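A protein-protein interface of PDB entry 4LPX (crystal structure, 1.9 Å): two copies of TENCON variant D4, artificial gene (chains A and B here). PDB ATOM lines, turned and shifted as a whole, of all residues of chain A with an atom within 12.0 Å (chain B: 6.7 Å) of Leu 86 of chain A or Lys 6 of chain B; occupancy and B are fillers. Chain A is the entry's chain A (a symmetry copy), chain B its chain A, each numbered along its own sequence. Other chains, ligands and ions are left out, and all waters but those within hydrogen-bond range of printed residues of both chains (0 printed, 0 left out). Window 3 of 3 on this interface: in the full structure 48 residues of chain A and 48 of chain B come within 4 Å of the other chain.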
ATOM      1  N   LEU A  82      12.213 -13.825  -6.356  1.00  0.00           N
ATOM      2  CA  LEU A  82      12.933 -12.771  -7.085  1.00  0.00           C
ATOM      3  C   LEU A  82      13.425 -11.723  -6.099  1.00  0.00           C
ATOM      4  O   LEU A  82      12.721 -11.402  -5.132  1.00  0.00           O
ATOM      5  CB  LEU A  82      12.016 -12.066  -8.085  1.00  0.00           C
ATOM      6  CG  LEU A  82      11.744 -12.517  -9.515  1.00  0.00           C
ATOM      7  CD1 LEU A  82      10.829 -11.505 -10.181  1.00  0.00           C
ATOM      8  CD2 LEU A  82      13.019 -12.669 -10.335  1.00  0.00           C
ATOM      9  N   SER A  83      14.622 -11.186  -6.330  1.00  0.00           N
ATOM     10  CA  SER A  83      15.073 -10.005  -5.589  1.00  0.00           C
ATOM     11  C   SER A  83      14.325  -8.771  -6.102  1.00  0.00           C
ATOM     12  O   SER A  83      13.606  -8.828  -7.106  1.00  0.00           O
ATOM     13  CB  SER A  83      16.577  -9.806  -5.766  1.00  0.00           C
ATOM     14  OG  SER A  83      16.853  -9.354  -7.087  1.00  0.00           O
ATOM     15  N   ASN A  84      14.492  -7.646  -5.412  1.00  0.00           N
ATOM     16  CA  ASN A  84      14.172  -6.353  -6.012  1.00  0.00           C
ATOM     17  C   ASN A  84      15.013  -6.166  -7.290  1.00  0.00           C
ATOM     18  O   ASN A  84      16.146  -6.646  -7.350  1.00  0.00           O
ATOM     19  CB  ASN A  84      14.471  -5.219  -5.022  1.00  0.00           C
ATOM     20  CG  ASN A  84      13.464  -5.150  -3.885  1.00  0.00           C
ATOM     21  OD1 ASN A  84      12.250  -5.226  -4.103  1.00  0.00           O
ATOM     22  ND2 ASN A  84      13.967  -5.009  -2.663  1.00  0.00           N
ATOM     23  N   PRO A  85      14.459  -5.474  -8.300  1.00  0.00           N
ATOM     24  CA  PRO A  85      15.229  -5.183  -9.513  1.00  0.00           C
ATOM     25  C   PRO A  85      16.282  -4.100  -9.305  1.00  0.00           C
ATOM     26  O   PRO A  85      16.108  -3.220  -8.472  1.00  0.00           O
ATOM     27  CB  PRO A  85      14.167  -4.705 -10.512  1.00  0.00           C
ATOM     28  CG  PRO A  85      13.061  -4.164  -9.666  1.00  0.00           C
ATOM     29  CD  PRO A  85      13.083  -4.938  -8.369  1.00  0.00           C
ATOM     30  N   LEU A  86      17.364  -4.183 -10.072  1.00  0.00           N
ATOM     31  CA  LEU A  86      18.296  -3.069 -10.220  1.00  0.00           C
ATOM     32  C   LEU A  86      18.207  -2.640 -11.680  1.00  0.00           C
ATOM     33  O   LEU A  86      18.337  -3.483 -12.590  1.00  0.00           O
ATOM     34  CB  LEU A  86      19.711  -3.479  -9.865  1.00  0.00           C
ATOM     35  CG  LEU A  86      20.762  -2.375 -10.086  1.00  0.00           C
ATOM     36  CD1 LEU A  86      20.468  -1.109  -9.266  1.00  0.00           C
ATOM     37  CD2 LEU A  86      22.099  -2.913  -9.753  1.00  0.00           C
ATOM     38  N   SER A  87      17.990  -1.344 -11.904  1.00  0.00           N
ATOM     39  CA  SER A  87      17.705  -0.832 -13.247  1.00  0.00           C
ATOM     40  C   SER A  87      18.714   0.219 -13.708  1.00  0.00           C
ATOM     41  O   SER A  87      19.321   0.908 -12.894  1.00  0.00           O
ATOM     42  CB  SER A  87      16.291  -0.245 -13.311  1.00  0.00           C
ATOM     43  OG  SER A  87      15.308  -1.261 -13.182  1.00  0.00           O
ATOM     44  N   ALA A  88      18.880   0.325 -15.024  1.00  0.00           N
ATOM     45  CA  ALA A  88      19.746   1.330 -15.624  1.00  0.00           C
ATOM     46  C   ALA A  88      19.232   1.634 -17.020  1.00  0.00           C
ATOM     47  O   ALA A  88      18.449   0.861 -17.580  1.00  0.00           O
ATOM     48  CB  ALA A  88      21.169   0.808 -15.700  1.00  0.00           C
ATOM     49  N   GLU A  89      19.671   2.761 -17.576  1.00  0.00           N
ATOM     50  CA  GLU A  89      19.395   3.084 -18.965  1.00  0.00           C
ATOM     51  C   GLU A  89      20.713   3.199 -19.696  1.00  0.00           C
ATOM     52  O   GLU A  89      21.532   4.069 -19.373  1.00  0.00           O
ATOM     53  CB  GLU A  89      18.621   4.402 -19.082  1.00  0.00           C
ATOM     54  CG  GLU A  89      17.271   4.398 -18.376  1.00  0.00           C
ATOM     55  CD  GLU A  89      16.642   5.778 -18.300  1.00  0.00           C
ATOM     56  OE1 GLU A  89      17.249   6.753 -18.799  1.00  0.00           O
ATOM     57  OE2 GLU A  89      15.533   5.882 -17.735  1.00  0.00           O
ATOM     58  N   PHE A  90      20.920   2.325 -20.678  1.00  0.00           N
ATOM     59  CA  PHE A  90      22.162   2.326 -21.437  1.00  0.00           C
ATOM     60  C   PHE A  90      21.876   2.595 -22.915  1.00  0.00           C
ATOM     61  O   PHE A  90      20.799   2.248 -23.421  1.00  0.00           O
ATOM     62  CB  PHE A  90      22.914   0.991 -21.304  1.00  0.00           C
ATOM     63  CG  PHE A  90      23.355   0.659 -19.897  1.00  0.00           C
ATOM     64  CD1 PHE A  90      24.030   1.603 -19.109  1.00  0.00           C
ATOM     65  CD2 PHE A  90      23.096  -0.610 -19.358  1.00  0.00           C
ATOM     66  CE1 PHE A  90      24.440   1.305 -17.816  1.00  0.00           C
ATOM     67  CE2 PHE A  90      23.507  -0.921 -18.054  1.00  0.00           C
ATOM     68  CZ  PHE A  90      24.180   0.035 -17.280  1.00  0.00           C
ATOM     69  N   ALA B   4      19.069  -7.291  -3.817  1.00  0.00           N
ATOM     70  CA  ALA B   4      19.250  -7.093  -5.254  1.00  0.00           C
ATOM     71  C   ALA B   4      20.725  -7.243  -5.675  1.00  0.00           C
ATOM     72  O   ALA B   4      21.627  -7.033  -4.854  1.00  0.00           O
ATOM     73  CB  ALA B   4      18.706  -5.721  -5.652  1.00  0.00           C
ATOM     74  N   PRO B   5      20.982  -7.609  -6.958  1.00  0.00           N
ATOM     75  CA  PRO B   5      22.360  -7.465  -7.453  1.00  0.00           C
ATOM     76  C   PRO B   5      22.753  -5.982  -7.341  1.00  0.00           C
ATOM     77  O   PRO B   5      21.870  -5.128  -7.197  1.00  0.00           O
ATOM     78  CB  PRO B   5      22.266  -7.866  -8.938  1.00  0.00           C
ATOM     79  CG  PRO B   5      20.941  -8.554  -9.109  1.00  0.00           C
ATOM     80  CD  PRO B   5      20.053  -8.144  -7.978  1.00  0.00           C
ATOM     81  N   LYS B   6      24.043  -5.676  -7.401  1.00  0.00           N
ATOM     82  CA  LYS B   6      24.502  -4.295  -7.208  1.00  0.00           C
ATOM     83  C   LYS B   6      25.268  -3.802  -8.432  1.00  0.00           C
ATOM     84  O   LYS B   6      25.808  -4.602  -9.189  1.00  0.00           O
ATOM     85  CB  LYS B   6      25.418  -4.195  -5.981  1.00  0.00           C
ATOM     86  CG  LYS B   6      24.833  -4.772  -4.693  1.00  0.00           C
ATOM     87  CD  LYS B   6      25.853  -4.747  -3.547  1.00  0.00           C
ATOM     88  CE  LYS B   6      27.058  -5.653  -3.809  1.00  0.00           C
ATOM     89  NZ  LYS B   6      28.047  -5.589  -2.689  1.00  0.00           N
ATOM     90  N   ASN B   7      25.313  -2.478  -8.619  1.00  0.00           N
ATOM     91  CA  ASN B   7      26.273  -1.867  -9.549  1.00  0.00           C
ATOM     92  C   ASN B   7      26.209  -2.403 -10.976  1.00  0.00           C
ATOM     93  O   ASN B   7      27.185  -2.948 -11.512  1.00  0.00           O
ATOM     94  CB  ASN B   7      27.711  -1.904  -8.980  1.00  0.00           C
ATOM     95  CG  ASN B   7      27.817  -1.154  -7.655  1.00  0.00           C
ATOM     96  OD1 ASN B   7      27.068  -0.216  -7.425  1.00  0.00           O
ATOM     97  ND2 ASN B   7      28.739  -1.563  -6.786  1.00  0.00           N
ATOM     98  N   LEU B   8      25.035  -2.236 -11.579  1.00  0.00           N
ATOM     99  CA  LEU B   8      24.834  -2.596 -12.969  1.00  0.00           C
ATOM    100  C   LEU B   8      25.529  -1.563 -13.850  1.00  0.00           C
ATOM    101  O   LEU B   8      25.206  -0.370 -13.801  1.00  0.00           O
ATOM    102  CB  LEU B   8      23.340  -2.682 -13.298  1.00  0.00           C
ATOM    103  CG  LEU B   8      22.954  -2.970 -14.758  1.00  0.00           C
ATOM    104  CD1 LEU B   8      23.491  -4.332 -15.267  1.00  0.00           C
ATOM    105  CD2 LEU B   8      21.449  -2.879 -14.882  1.00  0.00           C
ATOM    106  N   VAL B   9      26.479  -2.035 -14.646  1.00  0.00           N
ATOM    107  CA  VAL B   9      27.281  -1.166 -15.519  1.00  0.00           C
ATOM    108  C   VAL B   9      27.321  -1.691 -16.947  1.00  0.00           C
ATOM    109  O   VAL B   9      26.893  -2.824 -17.217  1.00  0.00           O
ATOM    110  CB  VAL B   9      28.724  -0.985 -14.975  1.00  0.00           C
ATOM    111  CG1 VAL B   9      28.688  -0.383 -13.562  1.00  0.00           C
ATOM    112  CG2 VAL B   9      29.503  -2.298 -14.990  1.00  0.00           C
ATOM    113  N   SER B  21      27.478  -5.710 -16.946  1.00  0.00           N
ATOM    114  CA  SER B  21      28.168  -6.345 -15.817  1.00  0.00           C
ATOM    115  C   SER B  21      27.509  -5.922 -14.506  1.00  0.00           C
ATOM    116  O   SER B  21      26.920  -4.843 -14.412  1.00  0.00           O
ATOM    117  CB  SER B  21      29.659  -5.981 -15.763  1.00  0.00           C
ATOM    118  OG  SER B  21      30.342  -6.387 -16.928  1.00  0.00           O
ATOM    119  N   TRP B  22      27.612  -6.773 -13.491  1.00  0.00           N
ATOM    120  CA  TRP B  22      27.016  -6.475 -12.186  1.00  0.00           C
ATOM    121  C   TRP B  22      27.796  -7.187 -11.079  1.00  0.00           C
ATOM    122  O   TRP B  22      28.672  -8.014 -11.356  1.00  0.00           O
ATOM    123  CB  TRP B  22      25.527  -6.877 -12.156  1.00  0.00           C
ATOM    124  CG  TRP B  22      25.304  -8.350 -12.454  1.00  0.00           C
ATOM    125  CD1 TRP B  22      25.203  -9.390 -11.541  1.00  0.00           C
ATOM    126  CD2 TRP B  22      25.159  -8.932 -13.745  1.00  0.00           C
ATOM    127  NE1 TRP B  22      25.000 -10.585 -12.210  1.00  0.00           N
ATOM    128  CE2 TRP B  22      24.971 -10.333 -13.559  1.00  0.00           C
ATOM    129  CE3 TRP B  22      25.167  -8.413 -15.056  1.00  0.00           C
ATOM    130  CZ2 TRP B  22      24.793 -11.212 -14.633  1.00  0.00           C
ATOM    131  CZ3 TRP B  22      24.990  -9.294 -16.129  1.00  0.00           C
ATOM    132  CH2 TRP B  22      24.805 -10.683 -15.902  1.00  0.00           C
ATOM    133  N   THR B  23      27.468  -6.856  -9.834  1.00  0.00           N
ATOM    134  CA  THR B  23      28.125  -7.460  -8.672  1.00  0.00           C
ATOM    135  C   THR B  23      27.070  -8.202  -7.840  1.00  0.00           C
ATOM    136  O   THR B  23      25.934  -7.729  -7.683  1.00  0.00           O
ATOM    137  CB  THR B  23      28.853  -6.390  -7.800  1.00  0.00           C
ATOM    138  OG1 THR B  23      29.858  -5.727  -8.591  1.00  0.00           O
ATOM    139  CG2 THR B  23      29.547  -7.040  -6.594  1.00  0.00           C
ATOM    140  N   ALA B  24      27.465  -9.358  -7.317  1.00  0.00           N
ATOM    141  CA  ALA B  24      26.632 -10.172  -6.425  1.00  0.00           C
ATOM    142  C   ALA B  24      26.526  -9.576  -5.017  1.00  0.00           C
ATOM    143  O   ALA B  24      27.508  -9.051  -4.480  1.00  0.00           O
ATOM    144  CB  ALA B  24      27.222 -11.565  -6.324  1.00  0.00           C
ATOM    145  N   PRO B  25      25.330  -9.654  -4.407  1.00  0.00           N
ATOM    146  CA  PRO B  25      25.190  -9.201  -3.029  1.00  0.00           C
ATOM    147  C   PRO B  25      25.681 -10.302  -2.072  1.00  0.00           C
ATOM    148  O   PRO B  25      26.387 -11.224  -2.505  1.00  0.00           O
ATOM    149  CB  PRO B  25      23.677  -8.976  -2.908  1.00  0.00           C
ATOM    150  CG  PRO B  25      23.101 -10.044  -3.768  1.00  0.00           C
ATOM    151  CD  PRO B  25      24.050 -10.162  -4.944  1.00  0.00           C
ATOM    152  N   ASP B  26      25.311 -10.203  -0.795  1.00  0.00           N
ATOM    153  CA  ASP B  26      25.654 -11.224   0.202  1.00  0.00           C
ATOM    154  C   ASP B  26      24.657 -12.395   0.183  1.00  0.00           C
ATOM    155  O   ASP B  26      24.298 -12.946   1.227  1.00  0.00           O
ATOM    156  CB  ASP B  26      25.748 -10.602   1.608  1.00  0.00           C
ATOM    157  CG  ASP B  26      26.557 -11.460   2.585  1.00  0.00           C
ATOM    158  OD1 ASP B  26      27.515 -12.139   2.152  1.00  0.00           O
ATOM    159  OD2 ASP B  26      26.229 -11.453   3.791  1.00  0.00           O
ATOM    160  N   VAL B  70      17.204  -1.325 -18.769  1.00  0.00           N
ATOM    161  CA  VAL B  70      17.659  -2.676 -18.404  1.00  0.00           C
ATOM    162  C   VAL B  70      17.370  -2.880 -16.926  1.00  0.00           C
ATOM    163  O   VAL B  70      17.729  -2.029 -16.098  1.00  0.00           O
ATOM    164  CB  VAL B  70      19.180  -2.840 -18.679  1.00  0.00           C
ATOM    165  CG1 VAL B  70      19.686  -4.228 -18.259  1.00  0.00           C
ATOM    166  CG2 VAL B  70      19.496  -2.573 -20.149  1.00  0.00           C
ATOM    167  N   SER B  71      16.723  -4.000 -16.589  1.00  0.00           N
ATOM    168  CA  SER B  71      16.524  -4.371 -15.190  1.00  0.00           C
ATOM    169  C   SER B  71      17.075  -5.776 -14.927  1.00  0.00           C
ATOM    170  O   SER B  71      16.889  -6.682 -15.742  1.00  0.00           O
ATOM    171  CB  SER B  71      15.029  -4.310 -14.816  1.00  0.00           C
ATOM    172  OG  SER B  71      14.545  -2.976 -14.867  1.00  0.00           O
ATOM    173  N   ILE B  72      17.747  -5.944 -13.794  1.00  0.00           N
ATOM    174  CA  ILE B  72      18.272  -7.260 -13.403  1.00  0.00           C
ATOM    175  C   ILE B  72      17.759  -7.650 -12.023  1.00  0.00           C
ATOM    176  O   ILE B  72      17.707  -6.802 -11.096  1.00  0.00           O
ATOM    177  CB  ILE B  72      19.832  -7.310 -13.473  1.00  0.00           C
ATOM    178  CG1 ILE B  72      20.345  -8.728 -13.179  1.00  0.00           C
ATOM    179  CG2 ILE B  72      20.479  -6.327 -12.494  1.00  0.00           C
ATOM    180  CD1 ILE B  72      21.772  -8.969 -13.626  1.00  0.00           C
ATOM    181  N   TYR B  73      17.380  -8.928 -11.887  1.00  0.00           N
ATOM    182  CA  TYR B  73      16.876  -9.470 -10.645  1.00  0.00           C
ATOM    183  C   TYR B  73      17.650 -10.742 -10.328  1.00  0.00           C
ATOM    184  O   TYR B  73      17.982 -11.507 -11.241  1.00  0.00           O
ATOM    185  CB  TYR B  73      15.433  -9.944 -10.798  1.00  0.00           C
ATOM    186  CG  TYR B  73      14.429  -8.990 -11.397  1.00  0.00           C
ATOM    187  CD1 TYR B  73      14.483  -8.630 -12.748  1.00  0.00           C
ATOM    188  CD2 TYR B  73      13.417  -8.448 -10.604  1.00  0.00           C
ATOM    189  CE1 TYR B  73      13.541  -7.741 -13.299  1.00  0.00           C
ATOM    190  CE2 TYR B  73      12.480  -7.568 -11.137  1.00  0.00           C
ATOM    191  CZ  TYR B  73      12.545  -7.220 -12.473  1.00  0.00           C
ATOM    192  OH  TYR B  73      11.610  -6.352 -12.971  1.00  0.00           O
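Among the printed residues, merely in contact across the chains: Leu 82 of chain A with Tyr 73 of chain B (3.7 Å), Ser 83 of chain A with Ala 4 of chain B (3.8 Å), Ser 83 of chain A with Pro 5 of chain B (3.5 Å), Ser 83 of chain A with Tyr 73 of chain B (3.5 Å), Asn 84 of chain A with Ala 4 of chain B (3.2 Å), Pro 85 of chain A with Ile 72 of chain B (3.4 Å), Pro 85 of chain A with Tyr 73 of chain B (3.4 Å), Leu 86 of chain A with Pro 5 of chain B (3.4 Å), Leu 86 of chain A with Lys 6 of chain B (3.5 Å), Leu 86 of chain A with Asn 7 of chain B (3.4 Å), Leu 86 of chain A with Leu 8 of chain B (3.5 Å), Leu 86 of chain A with Val 70 of chain B (3.8 Å), Leu 86 of chain A with Ser 71 of chain B (3.3 Å), Ser 87 of chain A with Val 70 of chain B (3.1 Å), Ala 88 of chain A with Leu 8 of chain B (3.8 Å), Phe 90 of chain A with Leu 8 of chain B (3.6 Å) and Phe 90 of chain A with Val 9 of chain B (3.6 Å).
Of chain B, only Pro 5 (3.4 Å), Lys 6 (3.5 Å), Asn 7 (3.4 Å), Leu 8 (3.5 Å), Val 70 (3.8 Å), Ser 71 (3.3 Å) and Ile 72 (2.8 Å) come within 4 Å of Leu 86 of chain A. Lys 6 of chain B touches just one residue of chain A: Leu 86 (3.5 Å). Of chain A, only Ser 83 (3.8 Å) and Asn 84 (3.2 Å) come within 4 Å of Ala 4 of chain B. Of chain A, only Ser 83 and Leu 86 come within 4 Å of Pro 5 of chain B. Asn 7 of chain B touches just one residue of chain A: Leu 86. Leu 8 of chain B touches three residues of chain A. No residue of chain A comes within 4 Å of Thr 23 of chain B. No residue of chain A comes within 4 Å of Ala 24 of chain B. No residue of chain A comes within 4 Å of Pro 25 of chain B. Val 70 of chain B touches just these residues of chain A: Leu 86, Ser 87 and Ala 88. Ser 71 of chain B touches two residues of chain A. Tyr 73 of chain B touches just these residues of chain A: Leu 82, Ser 83 and Pro 85. Printed residues of chain B within 4 Å of Phe 90 of chain A: Leu 8 and Val 9. Of the printed residues of chain B, Leu 82 of chain A touches Tyr 73 (3.7 Å). Ser 21 of chain B touches none of the printed residues of chain A. Asp 26 of chain B touches none of the printed residues of chain A.
Of the 9 printed residues of chain A, 8 touch a printed residue of chain B. Of the 16 printed residues of chain B, 10 touch a printed residue of chain A.
The side-chain hydroxyl of Ser 87 of chain A sits at hydrogen-bond distance from the side-chain hydroxyl of Ser 71 of chain B (2.5 Å). The backbone carbonyl oxygen (O) of Leu 86 of chain A is in hydrogen-bond range of the backbone NH (N) of Ile 72 of chain B (2.8 Å). N of Val 70 of chain B sits at hydrogen-bond distance from O of Ala 88 of chain A (2.8 Å).
O of Thr 23 of chain B is in hydrogen-bond range of N of Lys 6 of chain B. The backbone NH of Val 9 of chain B lies within hydrogen-bond range of the backbone carbonyl oxygen of Ser 21 of chain B, at 2.9 Å.
No position is printed for both chains.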
